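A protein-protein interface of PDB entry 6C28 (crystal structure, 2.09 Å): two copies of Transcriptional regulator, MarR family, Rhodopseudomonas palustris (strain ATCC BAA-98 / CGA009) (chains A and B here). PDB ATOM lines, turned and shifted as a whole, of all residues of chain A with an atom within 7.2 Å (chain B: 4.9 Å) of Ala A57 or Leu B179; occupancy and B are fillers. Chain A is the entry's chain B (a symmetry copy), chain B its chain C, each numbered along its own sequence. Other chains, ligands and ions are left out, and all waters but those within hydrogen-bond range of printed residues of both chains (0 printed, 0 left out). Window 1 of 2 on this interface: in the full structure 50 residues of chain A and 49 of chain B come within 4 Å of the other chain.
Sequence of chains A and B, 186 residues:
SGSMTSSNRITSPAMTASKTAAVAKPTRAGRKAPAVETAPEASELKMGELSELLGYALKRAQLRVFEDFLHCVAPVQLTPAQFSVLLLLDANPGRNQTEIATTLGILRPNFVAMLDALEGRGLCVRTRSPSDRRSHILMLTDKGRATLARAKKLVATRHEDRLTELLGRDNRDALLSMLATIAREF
The side-chain hydroxyl (OH) of Tyr A56 lies within hydrogen-bond range of the guanidinium group (NE) of Arg A60, at 3.2 Å. NZ of Lys A59 sits at hydrogen-bond distance from OE1 of Gln A62 (2.9 Å).
Among the printed residues, merely in contact across the chains: Leu A54 with Leu B175 (3.8 Å), Leu A54 with Leu B176 (3.8 Å), Ala A57 with Leu B176 (3.6 Å), Ala A57 with Leu B179 (3.8 Å), Leu A58 with Leu B58 (3.5 Å), Leu A58 with Leu B179 (3.9 Å), Arg A60 with Ala B183 (3.9 Å), Ala A61 with Leu B58 (3.8 Å), Ala A61 with Leu B179 (3.7 Å), Ala A61 with Ile B182 (3.9 Å), Gln A62 with Leu B58 (3.9 Å), Leu A175 with Leu B175 (3.2 Å), Leu A175 with Ile B182 (3.7 Å), Leu A179 with Leu B58 (3.7 Å) and Ile A182 with Leu B175 (3.8 Å).
Gly A55 touches none of the printed residues of chain B. Ala A57 touches two residues of chain B. Printed residues of chain B within 4 Å of Leu A58: Leu B58 and Leu B179. Printed residues of chain B within 4 Å of Ala A61: Leu B58 (3.8 Å), Leu B179 (3.7 Å) and Ile B182 (3.9 Å). Of the printed residues of chain B, Leu A175 touches Leu B175 and Ile B182. Of the printed residues of chain B, Leu A179 touches Leu B58 (3.7 Å). Met B178 touches none of the printed residues of chain A. Leu B179 touches just these residues of chain A: Ala A57, Leu A58 and Ala A61. The nearest printed residue of chain A that does not touch Leu B175 is Leu A179 (4.2 Å).
Of the 18 printed residues of chain A, 9 touch a printed residue of chain B. Printed residues of chain A that touch a printed residue of chain B: Leu A54, Ala A57, Leu A58, Arg A60, Ala A61, Gln A62, Leu A175, Leu A179 and Ile A182. Hydrophobic or aromatic side chains of chain A that line the printed part of chain B: Leu A54, Ala A57, Leu A58, Ala A61, Leu A175, Leu A179 and Ile A182. Along chain B the printed residues that touch a printed residue of chain A span positions 58 to 183. Among the printed residues, 15 pairs touch across the chains. Among the printed residues, no Asp or Glu carboxylate lies within 4 Å of a Lys or Arg side-chain nitrogen of the other chain.
Leu A58 touches its own counterpart, Leu B58. Leu A58 touches Leu B179, and with the chains exchanged Leu A179 touches Leu B58. Leu A175 touches its own counterpart, Leu B175. Leu A175 touches Ile B182, and with the chains exchanged Ile A182 touches Leu B175.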
ATOM      1  N   LEU A  50      11.874  23.135 -20.200  1.00  0.00           N
ATOM      2  CA  LEU A  50      11.323  21.811 -19.881  1.00  0.00           C
ATOM      3  C   LEU A  50      11.513  21.439 -18.440  1.00  0.00           C
ATOM      4  O   LEU A  50      10.603  20.890 -17.821  1.00  0.00           O
ATOM      5  CB  LEU A  50      11.954  20.736 -20.762  1.00  0.00           C
ATOM      6  CG  LEU A  50      11.233  20.091 -21.923  1.00  0.00           C
ATOM      7  CD1 LEU A  50       9.916  20.689 -22.346  1.00  0.00           C
ATOM      8  CD2 LEU A  50      12.187  19.916 -23.074  1.00  0.00           C
ATOM      9  N   SER A  51      12.663  21.784 -17.870  1.00  0.00           N
ATOM     10  CA  SER A  51      12.931  21.364 -16.487  1.00  0.00           C
ATOM     11  C   SER A  51      12.178  22.244 -15.471  1.00  0.00           C
ATOM     12  O   SER A  51      12.251  21.985 -14.293  1.00  0.00           O
ATOM     13  CB  SER A  51      14.434  21.366 -16.217  1.00  0.00           C
ATOM     14  OG  SER A  51      14.929  22.668 -16.390  1.00  0.00           O
ATOM     15  N   GLU A  52      11.436  23.256 -15.941  1.00  0.00           N
ATOM     16  CA  GLU A  52      10.565  24.080 -15.078  1.00  0.00           C
ATOM     17  C   GLU A  52       9.076  23.860 -15.355  1.00  0.00           C
ATOM     18  O   GLU A  52       8.243  24.557 -14.786  1.00  0.00           O
ATOM     19  CB  GLU A  52      10.919  25.562 -15.266  1.00  0.00           C
ATOM     20  CG  GLU A  52      12.406  25.878 -15.012  1.00  0.00           C
ATOM     21  CD  GLU A  52      12.924  25.417 -13.644  1.00  0.00           C
ATOM     22  OE1 GLU A  52      14.075  24.902 -13.553  1.00  0.00           O
ATOM     23  OE2 GLU A  52      12.167  25.555 -12.652  1.00  0.00           O
ATOM     24  N   LEU A  53       8.739  22.924 -16.242  1.00  0.00           N
ATOM     25  CA  LEU A  53       7.332  22.720 -16.643  1.00  0.00           C
ATOM     26  C   LEU A  53       6.806  21.503 -15.971  1.00  0.00           C
ATOM     27  O   LEU A  53       7.392  20.417 -16.080  1.00  0.00           O
ATOM     28  CB  LEU A  53       7.189  22.569 -18.142  1.00  0.00           C
ATOM     29  CG  LEU A  53       7.488  23.860 -18.870  1.00  0.00           C
ATOM     30  CD1 LEU A  53       7.514  23.664 -20.365  1.00  0.00           C
ATOM     31  CD2 LEU A  53       6.491  24.938 -18.530  1.00  0.00           C
ATOM     32  N   LEU A  54       5.702  21.684 -15.266  1.00  0.00           N
ATOM     33  CA  LEU A  54       5.110  20.636 -14.443  1.00  0.00           C
ATOM     34  C   LEU A  54       4.711  19.432 -15.312  1.00  0.00           C
ATOM     35  O   LEU A  54       4.914  18.314 -14.940  1.00  0.00           O
ATOM     36  CB  LEU A  54       3.904  21.205 -13.689  1.00  0.00           C
ATOM     37  CG  LEU A  54       3.508  20.658 -12.313  1.00  0.00           C
ATOM     38  CD1 LEU A  54       2.926  19.276 -12.420  1.00  0.00           C
ATOM     39  CD2 LEU A  54       4.685  20.616 -11.387  1.00  0.00           C
ATOM     40  N   GLY A  55       4.179  19.691 -16.494  1.00  0.00           N
ATOM     41  CA  GLY A  55       3.629  18.638 -17.353  1.00  0.00           C
ATOM     42  C   GLY A  55       4.717  17.667 -17.788  1.00  0.00           C
ATOM     43  O   GLY A  55       4.440  16.479 -17.992  1.00  0.00           O
ATOM     44  N   TYR A  56       5.949  18.206 -17.946  1.00  0.00           N
ATOM     45  CA  TYR A  56       7.072  17.437 -18.424  1.00  0.00           C
ATOM     46  C   TYR A  56       7.466  16.480 -17.312  1.00  0.00           C
ATOM     47  O   TYR A  56       7.710  15.303 -17.528  1.00  0.00           O
ATOM     48  CB  TYR A  56       8.236  18.326 -18.863  1.00  0.00           C
ATOM     49  CG  TYR A  56       9.421  17.512 -19.254  1.00  0.00           C
ATOM     50  CD1 TYR A  56       9.421  16.786 -20.448  1.00  0.00           C
ATOM     51  CD2 TYR A  56      10.524  17.432 -18.436  1.00  0.00           C
ATOM     52  CE1 TYR A  56      10.497  16.017 -20.817  1.00  0.00           C
ATOM     53  CE2 TYR A  56      11.630  16.646 -18.778  1.00  0.00           C
ATOM     54  CZ  TYR A  56      11.595  15.936 -19.973  1.00  0.00           C
ATOM     55  OH  TYR A  56      12.652  15.144 -20.318  1.00  0.00           O
ATOM     56  N   ALA A  57       7.558  17.018 -16.118  1.00  0.00           N
ATOM     57  CA  ALA A  57       8.011  16.236 -15.002  1.00  0.00           C
ATOM     58  C   ALA A  57       6.977  15.184 -14.660  1.00  0.00           C
ATOM     59  O   ALA A  57       7.287  14.077 -14.337  1.00  0.00           O
ATOM     60  CB  ALA A  57       8.235  17.155 -13.792  1.00  0.00           C
ATOM     61  N   LEU A  58       5.725  15.581 -14.711  1.00  0.00           N
ATOM     62  CA  LEU A  58       4.607  14.656 -14.550  1.00  0.00           C
ATOM     63  C   LEU A  58       4.673  13.489 -15.569  1.00  0.00           C
ATOM     64  O   LEU A  58       4.672  12.304 -15.202  1.00  0.00           O
ATOM     65  CB  LEU A  58       3.332  15.490 -14.670  1.00  0.00           C
ATOM     66  CG  LEU A  58       2.033  14.850 -14.373  1.00  0.00           C
ATOM     67  CD1 LEU A  58       2.075  14.209 -12.985  1.00  0.00           C
ATOM     68  CD2 LEU A  58       0.978  15.936 -14.487  1.00  0.00           C
ATOM     69  N   LYS A  59       4.857  13.818 -16.834  1.00  0.00           N
ATOM     70  CA  LYS A  59       4.998  12.791 -17.835  1.00  0.00           C
ATOM     71  C   LYS A  59       6.189  11.905 -17.596  1.00  0.00           C
ATOM     72  O   LYS A  59       6.050  10.702 -17.686  1.00  0.00           O
ATOM     73  CB  LYS A  59       5.071  13.369 -19.238  1.00  0.00           C
ATOM     74  CG  LYS A  59       5.145  12.369 -20.354  1.00  0.00           C
ATOM     75  CD  LYS A  59       4.081  11.281 -20.247  1.00  0.00           C
ATOM     76  CE  LYS A  59       4.011  10.413 -21.494  1.00  0.00           C
ATOM     77  NZ  LYS A  59       2.943   9.359 -21.427  1.00  0.00           N
ATOM     78  N   ARG A  60       7.349  12.441 -17.268  1.00  0.00           N
ATOM     79  CA  ARG A  60       8.517  11.602 -17.021  1.00  0.00           C
ATOM     80  C   ARG A  60       8.396  10.684 -15.808  1.00  0.00           C
ATOM     81  O   ARG A  60       8.867   9.589 -15.833  1.00  0.00           O
ATOM     82  CB  ARG A  60       9.769  12.421 -16.980  1.00  0.00           C
ATOM     83  CG  ARG A  60      10.095  12.960 -18.328  1.00  0.00           C
ATOM     84  CD  ARG A  60      10.298  11.826 -19.299  1.00  0.00           C
ATOM     85  NE  ARG A  60      11.414  12.171 -20.113  1.00  0.00           N
ATOM     86  CZ  ARG A  60      12.452  11.413 -20.352  1.00  0.00           C
ATOM     87  NH1 ARG A  60      13.397  11.900 -21.090  1.00  0.00           N
ATOM     88  NH2 ARG A  60      12.527  10.187 -19.910  1.00  0.00           N
ATOM     89  N   ALA A  61       7.800  11.174 -14.741  1.00  0.00           N
ATOM     90  CA  ALA A  61       7.519  10.361 -13.608  1.00  0.00           C
ATOM     91  C   ALA A  61       6.521   9.241 -13.941  1.00  0.00           C
ATOM     92  O   ALA A  61       6.690   8.078 -13.480  1.00  0.00           O
ATOM     93  CB  ALA A  61       6.992  11.229 -12.490  1.00  0.00           C
ATOM     94  N   GLN A  62       5.458   9.616 -14.687  1.00  0.00           N
ATOM     95  CA  GLN A  62       4.453   8.664 -15.128  1.00  0.00           C
ATOM     96  C   GLN A  62       5.067   7.507 -15.950  1.00  0.00           C
ATOM     97  O   GLN A  62       4.864   6.339 -15.650  1.00  0.00           O
ATOM     98  CB  GLN A  62       3.292   9.322 -15.851  1.00  0.00           C
ATOM     99  CG  GLN A  62       2.289   8.271 -16.354  1.00  0.00           C
ATOM    100  CD  GLN A  62       2.556   7.847 -17.764  1.00  0.00           C
ATOM    101  OE1 GLN A  62       2.765   8.698 -18.636  1.00  0.00           O
ATOM    102  NE2 GLN A  62       2.560   6.527 -18.021  1.00  0.00           N
ATOM    103  N   LEU A  63       5.928   7.847 -16.878  1.00  0.00           N
ATOM    104  CA  LEU A  63       6.639   6.889 -17.691  1.00  0.00           C
ATOM    105  C   LEU A  63       7.512   5.944 -16.865  1.00  0.00           C
ATOM    106  O   LEU A  63       7.523   4.760 -17.092  1.00  0.00           O
ATOM    107  CB  LEU A  63       7.492   7.622 -18.691  1.00  0.00           C
ATOM    108  CG  LEU A  63       7.116   7.745 -20.163  1.00  0.00           C
ATOM    109  CD1 LEU A  63       5.751   7.271 -20.588  1.00  0.00           C
ATOM    110  CD2 LEU A  63       7.412   9.116 -20.691  1.00  0.00           C
ATOM    111  N   LEU A 167      10.155   7.970  -1.434  1.00  0.00           N
ATOM    112  CA  LEU A 167       9.581   9.296  -1.248  1.00  0.00           C
ATOM    113  C   LEU A 167       9.435   9.667   0.222  1.00  0.00           C
ATOM    114  O   LEU A 167       9.507  10.842   0.584  1.00  0.00           O
ATOM    115  CB  LEU A 167       8.191   9.352  -1.902  1.00  0.00           C
ATOM    116  CG  LEU A 167       8.124   9.486  -3.422  1.00  0.00           C
ATOM    117  CD1 LEU A 167       6.700   9.279  -3.863  1.00  0.00           C
ATOM    118  CD2 LEU A 167       8.604  10.845  -3.903  1.00  0.00           C
ATOM    119  N   LEU A 175       1.793  14.119  -2.366  1.00  0.00           N
ATOM    120  CA  LEU A 175       1.892  13.930  -3.831  1.00  0.00           C
ATOM    121  C   LEU A 175       0.591  13.339  -4.365  1.00  0.00           C
ATOM    122  O   LEU A 175      -0.056  13.898  -5.272  1.00  0.00           O
ATOM    123  CB  LEU A 175       3.077  12.995  -4.201  1.00  0.00           C
ATOM    124  CG  LEU A 175       3.294  12.591  -5.649  1.00  0.00           C
ATOM    125  CD1 LEU A 175       3.484  13.825  -6.481  1.00  0.00           C
ATOM    126  CD2 LEU A 175       4.521  11.737  -5.774  1.00  0.00           C
ATOM    127  N   LEU A 179      -1.959  15.193  -6.971  1.00  0.00           N
ATOM    128  CA  LEU A 179      -2.271  14.507  -8.245  1.00  0.00           C
ATOM    129  C   LEU A 179      -3.750  14.343  -8.409  1.00  0.00           C
ATOM    130  O   LEU A 179      -4.305  14.629  -9.509  1.00  0.00           O
ATOM    131  CB  LEU A 179      -1.573  13.159  -8.344  1.00  0.00           C
ATOM    132  CG  LEU A 179      -0.042  13.257  -8.376  1.00  0.00           C
ATOM    133  CD1 LEU A 179       0.540  11.833  -8.342  1.00  0.00           C
ATOM    134  CD2 LEU A 179       0.423  14.094  -9.563  1.00  0.00           C
ATOM    135  N   ILE A 182      -5.274  17.599  -9.447  1.00  0.00           N
ATOM    136  CA  ILE A 182      -5.079  17.914 -10.886  1.00  0.00           C
ATOM    137  C   ILE A 182      -6.113  17.165 -11.701  1.00  0.00           C
ATOM    138  O   ILE A 182      -6.820  17.745 -12.509  1.00  0.00           O
ATOM    139  CB  ILE A 182      -3.644  17.576 -11.318  1.00  0.00           C
ATOM    140  CG1 ILE A 182      -2.691  18.558 -10.626  1.00  0.00           C
ATOM    141  CG2 ILE A 182      -3.496  17.635 -12.816  1.00  0.00           C
ATOM    142  CD1 ILE A 182      -1.269  18.119 -10.615  1.00  0.00           C
ATOM    143  N   LEU B  58      -0.997   9.345 -10.790  1.00  0.00           N
ATOM    144  CA  LEU B  58      -0.009   9.946 -11.665  1.00  0.00           C
ATOM    145  C   LEU B  58      -0.517   9.955 -13.119  1.00  0.00           C
ATOM    146  O   LEU B  58      -0.507  11.025 -13.796  1.00  0.00           O
ATOM    147  CB  LEU B  58       1.298   9.179 -11.518  1.00  0.00           C
ATOM    148  CG  LEU B  58       2.613   9.835 -11.855  1.00  0.00           C
ATOM    149  CD1 LEU B  58       2.770  11.250 -11.283  1.00  0.00           C
ATOM    150  CD2 LEU B  58       3.695   8.890 -11.339  1.00  0.00           C
ATOM    151  N   LEU B 175       5.741  19.731  -5.725  1.00  0.00           N
ATOM    152  CA  LEU B 175       5.254  18.681  -6.675  1.00  0.00           C
ATOM    153  C   LEU B 175       6.249  18.459  -7.783  1.00  0.00           C
ATOM    154  O   LEU B 175       6.607  17.317  -8.113  1.00  0.00           O
ATOM    155  CB  LEU B 175       3.934  19.086  -7.291  1.00  0.00           C
ATOM    156  CG  LEU B 175       3.324  18.120  -8.331  1.00  0.00           C
ATOM    157  CD1 LEU B 175       3.110  16.719  -7.773  1.00  0.00           C
ATOM    158  CD2 LEU B 175       2.004  18.718  -8.763  1.00  0.00           C
ATOM    159  N   LEU B 176       6.736  19.568  -8.331  1.00  0.00           N
ATOM    160  CA  LEU B 176       7.711  19.528  -9.387  1.00  0.00           C
ATOM    161  C   LEU B 176       8.889  18.720  -8.883  1.00  0.00           C
ATOM    162  O   LEU B 176       9.386  17.825  -9.594  1.00  0.00           O
ATOM    163  CB  LEU B 176       8.108  20.947  -9.846  1.00  0.00           C
ATOM    164  CG  LEU B 176       9.105  21.229 -10.960  1.00  0.00           C
ATOM    165  CD1 LEU B 176      10.556  21.003 -10.520  1.00  0.00           C
ATOM    166  CD2 LEU B 176       8.781  20.361 -12.158  1.00  0.00           C
ATOM    167  N   SER B 177       9.322  18.992  -7.661  1.00  0.00           N
ATOM    168  CA  SER B 177      10.583  18.409  -7.177  1.00  0.00           C
ATOM    169  C   SER B 177      10.409  16.921  -6.875  1.00  0.00           C
ATOM    170  O   SER B 177      11.269  16.119  -7.163  1.00  0.00           O
ATOM    171  CB  SER B 177      11.116  19.240  -5.967  1.00  0.00           C
ATOM    172  OG  SER B 177      11.668  18.448  -4.935  1.00  0.00           O
ATOM    173  N   MET B 178       9.264  16.553  -6.323  1.00  0.00           N
ATOM    174  CA  MET B 178       8.937  15.131  -6.116  1.00  0.00           C
ATOM    175  C   MET B 178       8.820  14.299  -7.440  1.00  0.00           C
ATOM    176  O   MET B 178       9.213  13.113  -7.502  1.00  0.00           O
ATOM    177  CB  MET B 178       7.641  14.987  -5.306  1.00  0.00           C
ATOM    178  CG  MET B 178       7.838  15.304  -3.854  1.00  0.00           C
ATOM    179  SD  MET B 178       6.452  14.793  -2.835  1.00  0.00           S
ATOM    180  CE  MET B 178       5.329  16.162  -3.090  1.00  0.00           C
ATOM    181  N   LEU B 179       8.277  14.917  -8.476  1.00  0.00           N
ATOM    182  CA  LEU B 179       8.143  14.248  -9.756  1.00  0.00           C
ATOM    183  C   LEU B 179       9.503  14.051 -10.350  1.00  0.00           C
ATOM    184  O   LEU B 179       9.815  12.956 -10.824  1.00  0.00           O
ATOM    185  CB  LEU B 179       7.257  15.021 -10.705  1.00  0.00           C
ATOM    186  CG  LEU B 179       5.796  15.095 -10.222  1.00  0.00           C
ATOM    187  CD1 LEU B 179       5.173  16.239 -10.935  1.00  0.00           C
ATOM    188  CD2 LEU B 179       5.002  13.817 -10.461  1.00  0.00           C
ATOM    189  N   ALA B 180      10.332  15.092 -10.304  1.00  0.00           N
ATOM    190  CA  ALA B 180      11.719  14.970 -10.785  1.00  0.00           C
ATOM    191  C   ALA B 180      12.478  13.898 -10.034  1.00  0.00           C
ATOM    192  O   ALA B 180      13.303  13.195 -10.622  1.00  0.00           O
ATOM    193  CB  ALA B 180      12.457  16.294 -10.652  1.00  0.00           C
ATOM    194  N   THR B 181      12.225  13.758  -8.738  1.00  0.00           N
ATOM    195  CA  THR B 181      12.860  12.663  -7.953  1.00  0.00           C
ATOM    196  C   THR B 181      12.447  11.257  -8.438  1.00  0.00           C
ATOM    197  O   THR B 181      13.292  10.347  -8.566  1.00  0.00           O
ATOM    198  CB  THR B 181      12.478  12.774  -6.478  1.00  0.00           C
ATOM    199  OG1 THR B 181      12.846  14.072  -6.002  1.00  0.00           O
ATOM    200  CG2 THR B 181      13.118  11.657  -5.620  1.00  0.00           C
ATOM    201  N   ILE B 182      11.151  11.092  -8.724  1.00  0.00           N
ATOM    202  CA  ILE B 182      10.644   9.822  -9.245  1.00  0.00           C
ATOM    203  C   ILE B 182      11.295   9.487 -10.585  1.00  0.00           C
ATOM    204  O   ILE B 182      11.814   8.374 -10.787  1.00  0.00           O
ATOM    205  CB  ILE B 182       9.116   9.838  -9.372  1.00  0.00           C
ATOM    206  CG1 ILE B 182       8.500   9.862  -7.976  1.00  0.00           C
ATOM    207  CG2 ILE B 182       8.638   8.589 -10.120  1.00  0.00           C
ATOM    208  CD1 ILE B 182       7.037  10.211  -7.977  1.00  0.00           C
ATOM    209  N   ALA B 183      11.305  10.471 -11.479  1.00  0.00           N
ATOM    210  CA  ALA B 183      11.923  10.305 -12.801  1.00  0.00           C
ATOM    211  C   ALA B 183      13.433  10.000 -12.686  1.00  0.00           C
ATOM    212  O   ALA B 183      13.998   9.255 -13.481  1.00  0.00           O
ATOM    213  CB  ALA B 183      11.667  11.553 -13.673  1.00  0.00           C
